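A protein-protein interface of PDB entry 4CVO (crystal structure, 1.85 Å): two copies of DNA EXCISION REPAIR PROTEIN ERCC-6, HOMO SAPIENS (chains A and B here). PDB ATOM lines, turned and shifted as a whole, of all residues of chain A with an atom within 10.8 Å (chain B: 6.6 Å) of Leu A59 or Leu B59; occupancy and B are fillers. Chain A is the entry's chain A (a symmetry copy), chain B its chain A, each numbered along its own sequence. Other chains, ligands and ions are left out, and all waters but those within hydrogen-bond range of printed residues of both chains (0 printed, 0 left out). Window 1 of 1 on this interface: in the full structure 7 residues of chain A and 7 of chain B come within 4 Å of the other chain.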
ATOM      1  N   LYS A  50      -0.890  25.755 -16.337  1.00  0.00           N
ATOM      2  CA  LYS A  50      -1.665  26.529 -15.369  1.00  0.00           C
ATOM      3  C   LYS A  50      -2.449  27.653 -16.043  1.00  0.00           C
ATOM      4  O   LYS A  50      -3.618  27.893 -15.720  1.00  0.00           O
ATOM      5  CB  LYS A  50      -0.753  27.114 -14.290  1.00  0.00           C
ATOM      6  CG  LYS A  50      -0.190  26.085 -13.325  1.00  0.00           C
ATOM      7  N   GLU A  51      -1.801  28.342 -16.976  1.00  0.00           N
ATOM      8  CA  GLU A  51      -2.426  29.457 -17.681  1.00  0.00           C
ATOM      9  C   GLU A  51      -3.586  29.003 -18.559  1.00  0.00           C
ATOM     10  O   GLU A  51      -4.627  29.664 -18.623  1.00  0.00           O
ATOM     11  CB  GLU A  51      -1.387  30.196 -18.528  1.00  0.00           C
ATOM     12  CG  GLU A  51      -0.882  31.471 -17.883  1.00  0.00           C
ATOM     13  CD  GLU A  51      -2.011  32.434 -17.567  1.00  0.00           C
ATOM     14  OE1 GLU A  51      -2.887  32.629 -18.437  1.00  0.00           O
ATOM     15  OE2 GLU A  51      -2.028  32.988 -16.447  1.00  0.00           O
ATOM     16  N   TYR A  52      -3.403  27.877 -19.236  1.00  0.00           N
ATOM     17  CA  TYR A  52      -4.458  27.305 -20.059  1.00  0.00           C
ATOM     18  C   TYR A  52      -5.624  26.842 -19.194  1.00  0.00           C
ATOM     19  O   TYR A  52      -6.790  27.108 -19.506  1.00  0.00           O
ATOM     20  CB  TYR A  52      -3.923  26.139 -20.893  1.00  0.00           C
ATOM     21  CG  TYR A  52      -5.000  25.401 -21.658  1.00  0.00           C
ATOM     22  CD1 TYR A  52      -5.447  25.866 -22.889  1.00  0.00           C
ATOM     23  CD2 TYR A  52      -5.572  24.240 -21.149  1.00  0.00           C
ATOM     24  CE1 TYR A  52      -6.425  25.195 -23.590  1.00  0.00           C
ATOM     25  CE2 TYR A  52      -6.559  23.566 -21.845  1.00  0.00           C
ATOM     26  CZ  TYR A  52      -6.979  24.047 -23.064  1.00  0.00           C
ATOM     27  OH  TYR A  52      -7.960  23.375 -23.761  1.00  0.00           O
ATOM     28  N   ARG A  53      -5.300  26.147 -18.107  1.00  0.00           N
ATOM     29  CA  ARG A  53      -6.311  25.637 -17.185  1.00  0.00           C
ATOM     30  C   ARG A  53      -7.178  26.752 -16.602  1.00  0.00           C
ATOM     31  O   ARG A  53      -8.403  26.616 -16.506  1.00  0.00           O
ATOM     32  CB  ARG A  53      -5.646  24.855 -16.051  1.00  0.00           C
ATOM     33  CG  ARG A  53      -6.617  24.391 -14.982  1.00  0.00           C
ATOM     34  CD  ARG A  53      -7.619  23.401 -15.551  1.00  0.00           C
ATOM     35  NE  ARG A  53      -7.125  22.029 -15.484  1.00  0.00           N
ATOM     36  CZ  ARG A  53      -7.592  21.110 -14.644  1.00  0.00           C
ATOM     37  NH1 ARG A  53      -8.578  21.411 -13.807  1.00  0.00           N
ATOM     38  NH2 ARG A  53      -7.081  19.886 -14.647  1.00  0.00           N
ATOM     39  N   SER A  54      -6.541  27.852 -16.217  1.00  0.00           N
ATOM     40  CA  SER A  54      -7.253  28.986 -15.637  1.00  0.00           C
ATOM     41  C   SER A  54      -8.281  29.554 -16.611  1.00  0.00           C
ATOM     42  O   SER A  54      -9.375  29.964 -16.213  1.00  0.00           O
ATOM     43  CB  SER A  54      -6.264  30.073 -15.221  1.00  0.00           C
ATOM     44  OG  SER A  54      -6.923  31.127 -14.546  1.00  0.00           O
ATOM     45  N   VAL A  55      -7.924  29.573 -17.891  1.00  0.00           N
ATOM     46  CA  VAL A  55      -8.827  30.048 -18.929  1.00  0.00           C
ATOM     47  C   VAL A  55      -9.929  29.024 -19.169  1.00  0.00           C
ATOM     48  O   VAL A  55     -11.103  29.380 -19.301  1.00  0.00           O
ATOM     49  CB  VAL A  55      -8.075  30.331 -20.245  1.00  0.00           C
ATOM     50  CG1 VAL A  55      -9.049  30.682 -21.354  1.00  0.00           C
ATOM     51  CG2 VAL A  55      -7.064  31.450 -20.042  1.00  0.00           C
ATOM     52  N   LEU A  56      -9.548  27.751 -19.203  1.00  0.00           N
ATOM     53  CA  LEU A  56     -10.508  26.670 -19.396  1.00  0.00           C
ATOM     54  C   LEU A  56     -11.557  26.625 -18.279  1.00  0.00           C
ATOM     55  O   LEU A  56     -12.737  26.390 -18.545  1.00  0.00           O
ATOM     56  CB  LEU A  56      -9.787  25.325 -19.492  1.00  0.00           C
ATOM     57  CG  LEU A  56     -10.643  24.133 -19.918  1.00  0.00           C
ATOM     58  CD1 LEU A  56     -11.437  24.470 -21.168  1.00  0.00           C
ATOM     59  CD2 LEU A  56      -9.763  22.918 -20.158  1.00  0.00           C
ATOM     60  N   ASP A  57     -11.136  26.859 -17.038  1.00  0.00           N
ATOM     61  CA  ASP A  57     -12.077  26.904 -15.917  1.00  0.00           C
ATOM     62  C   ASP A  57     -13.029  28.088 -16.051  1.00  0.00           C
ATOM     63  O   ASP A  57     -14.234  27.970 -15.793  1.00  0.00           O
ATOM     64  CB  ASP A  57     -11.336  26.987 -14.580  1.00  0.00           C
ATOM     65  CG  ASP A  57     -10.426  25.794 -14.334  1.00  0.00           C
ATOM     66  OD1 ASP A  57     -10.684  24.709 -14.897  1.00  0.00           O
ATOM     67  OD2 ASP A  57      -9.449  25.941 -13.570  1.00  0.00           O
ATOM     68  N   ASP A  58     -12.485  29.236 -16.448  1.00  0.00           N
ATOM     69  CA  ASP A  58     -13.299  30.433 -16.660  1.00  0.00           C
ATOM     70  C   ASP A  58     -14.340  30.224 -17.750  1.00  0.00           C
ATOM     71  O   ASP A  58     -15.491  30.674 -17.629  1.00  0.00           O
ATOM     72  CB  ASP A  58     -12.412  31.627 -17.016  1.00  0.00           C
ATOM     73  CG  ASP A  58     -11.698  32.204 -15.810  1.00  0.00           C
ATOM     74  OD1 ASP A  58     -11.651  31.523 -14.766  1.00  0.00           O
ATOM     75  OD2 ASP A  58     -11.185  33.340 -15.906  1.00  0.00           O
ATOM     76  N   LEU A  59     -13.938  29.557 -18.824  1.00  0.00           N
ATOM     77  CA  LEU A  59     -14.855  29.278 -19.921  1.00  0.00           C
ATOM     78  C   LEU A  59     -15.924  28.300 -19.461  1.00  0.00           C
ATOM     79  O   LEU A  59     -17.097  28.438 -19.809  1.00  0.00           O
ATOM     80  CB  LEU A  59     -14.106  28.723 -21.133  1.00  0.00           C
ATOM     81  CG  LEU A  59     -14.986  28.285 -22.305  1.00  0.00           C
ATOM     82  CD1 LEU A  59     -15.856  29.434 -22.815  1.00  0.00           C
ATOM     83  CD2 LEU A  59     -14.136  27.713 -23.429  1.00  0.00           C
ATOM     84  N   THR A  60     -15.517  27.319 -18.663  1.00  0.00           N
ATOM     85  CA  THR A  60     -16.464  26.372 -18.085  1.00  0.00           C
ATOM     86  C   THR A  60     -17.478  27.081 -17.189  1.00  0.00           C
ATOM     87  O   THR A  60     -18.676  26.823 -17.274  1.00  0.00           O
ATOM     88  CB  THR A  60     -15.744  25.281 -17.275  1.00  0.00           C
ATOM     89  OG1 THR A  60     -15.074  24.392 -18.172  1.00  0.00           O
ATOM     90  CG2 THR A  60     -16.739  24.478 -16.450  1.00  0.00           C
ATOM     91  N   SER A  61     -16.993  27.979 -16.337  1.00  0.00           N
ATOM     92  CA  SER A  61     -17.862  28.721 -15.427  1.00  0.00           C
ATOM     93  C   SER A  61     -18.830  29.631 -16.173  1.00  0.00           C
ATOM     94  O   SER A  61     -20.007  29.739 -15.805  1.00  0.00           O
ATOM     95  CB  SER A  61     -17.027  29.545 -14.449  1.00  0.00           C
ATOM     96  OG  SER A  61     -16.239  28.700 -13.635  1.00  0.00           O
ATOM     97  N   CYS A  62     -18.341  30.294 -17.214  1.00  0.00           N
ATOM     98  CA  CYS A  62     -19.201  31.185 -17.988  1.00  0.00           C
ATOM     99  C   CYS A  62     -20.278  30.389 -18.730  1.00  0.00           C
ATOM    100  O   CYS A  62     -21.445  30.806 -18.808  1.00  0.00           O
ATOM    101  CB  CYS A  62     -18.376  32.017 -18.976  1.00  0.00           C
ATOM    102  SG  CYS A  62     -19.338  33.331 -19.771  1.00  0.00           S
ATOM    103  N   THR A  63     -19.882  29.233 -19.253  1.00  0.00           N
ATOM    104  CA  THR A  63     -20.779  28.388 -20.034  1.00  0.00           C
ATOM    105  C   THR A  63     -21.926  27.844 -19.191  1.00  0.00           C
ATOM    106  O   THR A  63     -23.093  27.960 -19.571  1.00  0.00           O
ATOM    107  CB  THR A  63     -20.021  27.204 -20.672  1.00  0.00           C
ATOM    108  OG1 THR A  63     -19.065  27.705 -21.611  1.00  0.00           O
ATOM    109  CG2 THR A  63     -20.987  26.275 -21.393  1.00  0.00           C
ATOM    110  N   THR A  64     -21.595  27.257 -18.045  1.00  0.00           N
ATOM    111  CA  THR A  64     -22.609  26.669 -17.179  1.00  0.00           C
ATOM    112  C   THR A  64     -23.596  27.733 -16.694  1.00  0.00           C
ATOM    113  O   THR A  64     -24.777  27.446 -16.500  1.00  0.00           O
ATOM    114  CB  THR A  64     -21.976  25.937 -15.969  1.00  0.00           C
ATOM    115  OG1 THR A  64     -23.011  25.485 -15.087  1.00  0.00           O
ATOM    116  CG2 THR A  64     -21.033  26.847 -15.207  1.00  0.00           C
ATOM    117  N   SER A  65     -23.121  28.965 -16.529  1.00  0.00           N
ATOM    118  CA  SER A  65     -24.016  30.070 -16.189  1.00  0.00           C
ATOM    119  C   SER A  65     -25.069  30.281 -17.272  1.00  0.00           C
ATOM    120  O   SER A  65     -26.267  30.424 -16.971  1.00  0.00           O
ATOM    121  CB  SER A  65     -23.230  31.362 -15.974  1.00  0.00           C
ATOM    122  OG  SER A  65     -22.468  31.299 -14.782  1.00  0.00           O
ATOM    123  N   LEU A  66     -24.625  30.301 -18.527  1.00  0.00           N
ATOM    124  CA  LEU A  66     -25.542  30.487 -19.653  1.00  0.00           C
ATOM    125  C   LEU A  66     -26.596  29.387 -19.703  1.00  0.00           C
ATOM    126  O   LEU A  66     -27.760  29.646 -19.992  1.00  0.00           O
ATOM    127  CB  LEU A  66     -24.777  30.525 -20.976  1.00  0.00           C
ATOM    128  CG  LEU A  66     -23.767  31.657 -21.164  1.00  0.00           C
ATOM    129  CD1 LEU A  66     -23.212  31.636 -22.581  1.00  0.00           C
ATOM    130  CD2 LEU A  66     -24.408  32.993 -20.858  1.00  0.00           C
ATOM    131  N   ARG A  67     -26.168  28.161 -19.428  1.00  0.00           N
ATOM    132  CA  ARG A  67     -27.064  27.016 -19.341  1.00  0.00           C
ATOM    133  C   ARG A  67     -28.091  27.241 -18.240  1.00  0.00           C
ATOM    134  O   ARG A  67     -29.276  26.955 -18.416  1.00  0.00           O
ATOM    135  CB  ARG A  67     -26.262  25.735 -19.081  1.00  0.00           C
ATOM    136  CG  ARG A  67     -27.108  24.483 -18.902  1.00  0.00           C
ATOM    137  CD  ARG A  67     -27.112  24.009 -17.453  1.00  0.00           C
ATOM    138  NE  ARG A  67     -25.788  23.596 -17.000  1.00  0.00           N
ATOM    139  CZ  ARG A  67     -25.517  23.165 -15.771  1.00  0.00           C
ATOM    140  NH1 ARG A  67     -26.480  23.088 -14.863  1.00  0.00           N
ATOM    141  NH2 ARG A  67     -24.282  22.811 -15.449  1.00  0.00           N
ATOM    142  N   SER B  54      -8.354  29.321 -29.363  1.00  0.00           N
ATOM    143  CA  SER B  54      -9.743  28.927 -29.571  1.00  0.00           C
ATOM    144  C   SER B  54     -10.542  29.001 -28.273  1.00  0.00           C
ATOM    145  O   SER B  54     -11.715  29.388 -28.269  1.00  0.00           O
ATOM    146  CB  SER B  54      -9.809  27.515 -30.150  1.00  0.00           C
ATOM    147  OG  SER B  54     -11.141  27.161 -30.472  1.00  0.00           O
ATOM    148  N   VAL B  55      -9.900  28.631 -27.170  1.00  0.00           N
ATOM    149  CA  VAL B  55     -10.531  28.695 -25.860  1.00  0.00           C
ATOM    150  C   VAL B  55     -10.640  30.145 -25.406  1.00  0.00           C
ATOM    151  O   VAL B  55     -11.675  30.567 -24.882  1.00  0.00           O
ATOM    152  CB  VAL B  55      -9.750  27.873 -24.816  1.00  0.00           C
ATOM    153  CG1 VAL B  55     -10.335  28.070 -23.431  1.00  0.00           C
ATOM    154  CG2 VAL B  55      -9.754  26.399 -25.198  1.00  0.00           C
ATOM    155  N   LEU B  56      -9.576  30.909 -25.628  1.00  0.00           N
ATOM    156  CA  LEU B  56      -9.560  32.323 -25.268  1.00  0.00           C
ATOM    157  C   LEU B  56     -10.642  33.118 -26.007  1.00  0.00           C
ATOM    158  O   LEU B  56     -11.281  33.992 -25.419  1.00  0.00           O
ATOM    159  CB  LEU B  56      -8.184  32.930 -25.544  1.00  0.00           C
ATOM    160  CG  LEU B  56      -7.953  34.342 -25.007  1.00  0.00           C
ATOM    161  CD1 LEU B  56      -8.356  34.427 -23.544  1.00  0.00           C
ATOM    162  CD2 LEU B  56      -6.496  34.735 -25.180  1.00  0.00           C
ATOM    163  N   ASP B  57     -10.858  32.812 -27.284  1.00  0.00           N
ATOM    164  CA  ASP B  57     -11.918  33.470 -28.051  1.00  0.00           C
ATOM    165  C   ASP B  57     -13.294  33.105 -27.504  1.00  0.00           C
ATOM    166  O   ASP B  57     -14.182  33.960 -27.391  1.00  0.00           O
ATOM    167  CB  ASP B  57     -11.836  33.098 -29.534  1.00  0.00           C
ATOM    168  CG  ASP B  57     -10.519  33.507 -30.174  1.00  0.00           C
ATOM    169  OD1 ASP B  57      -9.874  34.456 -29.680  1.00  0.00           O
ATOM    170  OD2 ASP B  57     -10.129  32.880 -31.181  1.00  0.00           O
ATOM    171  N   ASP B  58     -13.473  31.829 -27.171  1.00  0.00           N
ATOM    172  CA  ASP B  58     -14.732  31.361 -26.592  1.00  0.00           C
ATOM    173  C   ASP B  58     -15.032  32.042 -25.265  1.00  0.00           C
ATOM    174  O   ASP B  58     -16.185  32.403 -24.978  1.00  0.00           O
ATOM    175  CB  ASP B  58     -14.702  29.844 -26.399  1.00  0.00           C
ATOM    176  CG  ASP B  58     -14.901  29.086 -27.696  1.00  0.00           C
ATOM    177  OD1 ASP B  58     -14.772  29.706 -28.772  1.00  0.00           O
ATOM    178  OD2 ASP B  58     -15.188  27.871 -27.641  1.00  0.00           O
ATOM    179  N   LEU B  59     -14.002  32.205 -24.445  1.00  0.00           N
ATOM    180  CA  LEU B  59     -14.166  32.864 -23.156  1.00  0.00           C
ATOM    181  C   LEU B  59     -14.494  34.334 -23.369  1.00  0.00           C
ATOM    182  O   LEU B  59     -15.329  34.902 -22.664  1.00  0.00           O
ATOM    183  CB  LEU B  59     -12.909  32.713 -22.299  1.00  0.00           C
ATOM    184  CG  LEU B  59     -12.926  33.467 -20.968  1.00  0.00           C
ATOM    185  CD1 LEU B  59     -14.106  33.039 -20.095  1.00  0.00           C
ATOM    186  CD2 LEU B  59     -11.612  33.278 -20.228  1.00  0.00           C
ATOM    187  N   THR B  60     -13.843  34.943 -24.354  1.00  0.00           N
ATOM    188  CA  THR B  60     -14.137  36.326 -24.712  1.00  0.00           C
ATOM    189  C   THR B  60     -15.585  36.483 -25.172  1.00  0.00           C
ATOM    190  O   THR B  60     -16.278  37.407 -24.752  1.00  0.00           O
ATOM    191  CB  THR B  60     -13.194  36.832 -25.817  1.00  0.00           C
ATOM    192  OG1 THR B  60     -11.887  37.025 -25.270  1.00  0.00           O
ATOM    193  CG2 THR B  60     -13.686  38.158 -26.378  1.00  0.00           C
ATOM    194  N   SER B  61     -16.038  35.574 -26.029  1.00  0.00           N
ATOM    195  CA  SER B  61     -17.405  35.619 -26.543  1.00  0.00           C
ATOM    196  C   SER B  61     -18.438  35.413 -25.443  1.00  0.00           C
ATOM    197  O   SER B  61     -19.478  36.084 -25.418  1.00  0.00           O
ATOM    198  CB  SER B  61     -17.597  34.568 -27.635  1.00  0.00           C
ATOM    199  OG  SER B  61     -16.755  34.840 -28.738  1.00  0.00           O
ATOM    200  N   CYS B  62     -18.165  34.482 -24.536  1.00  0.00           N
ATOM    201  CA  CYS B  62     -19.100  34.222 -23.444  1.00  0.00           C
ATOM    202  C   CYS B  62     -19.175  35.423 -22.499  1.00  0.00           C
ATOM    203  O   CYS B  62     -20.258  35.798 -22.022  1.00  0.00           O
ATOM    204  CB  CYS B  62     -18.700  32.959 -22.673  1.00  0.00           C
ATOM    205  SG  CYS B  62     -19.960  32.427 -21.485  1.00  0.00           S
ATOM    206  N   THR B  63     -18.021  36.034 -22.250  1.00  0.00           N
ATOM    207  CA  THR B  63     -17.922  37.160 -21.328  1.00  0.00           C
ATOM    208  C   THR B  63     -18.688  38.377 -21.831  1.00  0.00           C
ATOM    209  O   THR B  63     -19.496  38.956 -21.101  1.00  0.00           O
ATOM    210  CB  THR B  63     -16.451  37.559 -21.085  1.00  0.00           C
ATOM    211  OG1 THR B  63     -15.769  36.482 -20.436  1.00  0.00           O
ATOM    212  CG2 THR B  63     -16.371  38.800 -20.207  1.00  0.00           C
ATOM    213  N   THR B  64     -18.440  38.761 -23.080  1.00  0.00           N
ATOM    214  CA  THR B  64     -19.090  39.934 -23.652  1.00  0.00           C
ATOM    215  C   THR B  64     -20.608  39.751 -23.692  1.00  0.00           C
ATOM    216  O   THR B  64     -21.356  40.717 -23.544  1.00  0.00           O
ATOM    217  CB  THR B  64     -18.552  40.254 -25.068  1.00  0.00           C
ATOM    218  OG1 THR B  64     -19.304  41.334 -25.634  1.00  0.00           O
ATOM    219  CG2 THR B  64     -18.651  39.046 -25.981  1.00  0.00           C
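Val A55 touches its own counterpart, Val B55. Val A55 touches Leu B59, and with the chains exchanged Leu A59 touches Val B55. Asp A58 touches Leu B59, and with the chains exchanged Leu A59 touches Asp B58. Cys A62 touches Thr B63, and with the chains exchanged Thr A63 touches Cys B62. 11 positions are printed for both chains.
The backbone carbonyl oxygen (O) of Leu A59 is in hydrogen-bond range of the side-chain hydroxyl (OG1) of Thr A63 (2.8 Å). O of Leu B59 is in hydrogen-bond range of OG1 of Thr B63.
Printed residues of chain B that touch a printed residue of chain A: Val B55, Asp B58, Leu B59, Cys B62 and Thr B63. Along chain B the printed residues that touch a printed residue of chain A span positions 55 to 63. Hydrophobic or aromatic side chains of chain A that line the printed part of chain B: Tyr A52, Val A55, Leu A59 and Leu A66. Among the printed residues, 11 pairs touch across the chains. Among the printed residues, no Asp or Glu carboxylate lies within 4 Å of a Lys or Arg side-chain nitrogen of the other chain.
Among the printed residues, merely in contact across the chains: Leu A66 with Cys B62, Val A55 with Val B55, Asp A58 with Leu B59, Leu A59 with Asp B58, Leu A59 with Leu B59, Tyr A52 with Val B55, Leu A59 with Val B55, Val A55 with Leu B59, Cys A62 with Thr B63 and Thr A63 with Cys B62.
SG of Cys B62 is disulfide-bonded to SG of Cys A62, 2.0 Å away.
Lys A50 touches none of the printed residues of chain B. Of the printed residues of chain B, Tyr A52 touches Val B55. Arg A53 touches none of the printed residues of chain B. Of the printed residues of chain B, Asp A58 touches Leu B59. Leu A59 touches just these residues of chain B: Val B55 (3.8 Å), Asp B58 (3.7 Å) and Leu B59 (3.7 Å). Printed residues of chain B within 4 Å of Leu A66: Cys B62 (3.5 Å). Val B55 touches just these residues of chain A: Tyr A52 (3.8 Å), Val A55 (3.6 Å) and Leu A59 (3.8 Å). Of chain A, only Leu A59 comes within 4 Å of Asp B58. Of chain A, only Val A55, Asp A58 and Leu A59 come within 4 Å of Leu B59. No residue of chain A comes within 4 Å of Thr B60. Ser B61 touches none of the printed residues of chain A. Cys B62 touches three residues of chain A. Of chain A, only Cys A62 (3.9 Å) comes within 4 Å of Thr B63. The nearest residue of chain B that does not touch Leu A59 is Cys B62 (4.5 Å). The nearest residue of chain A that does not touch Leu B59 is Cys A62 (4.5 Å).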
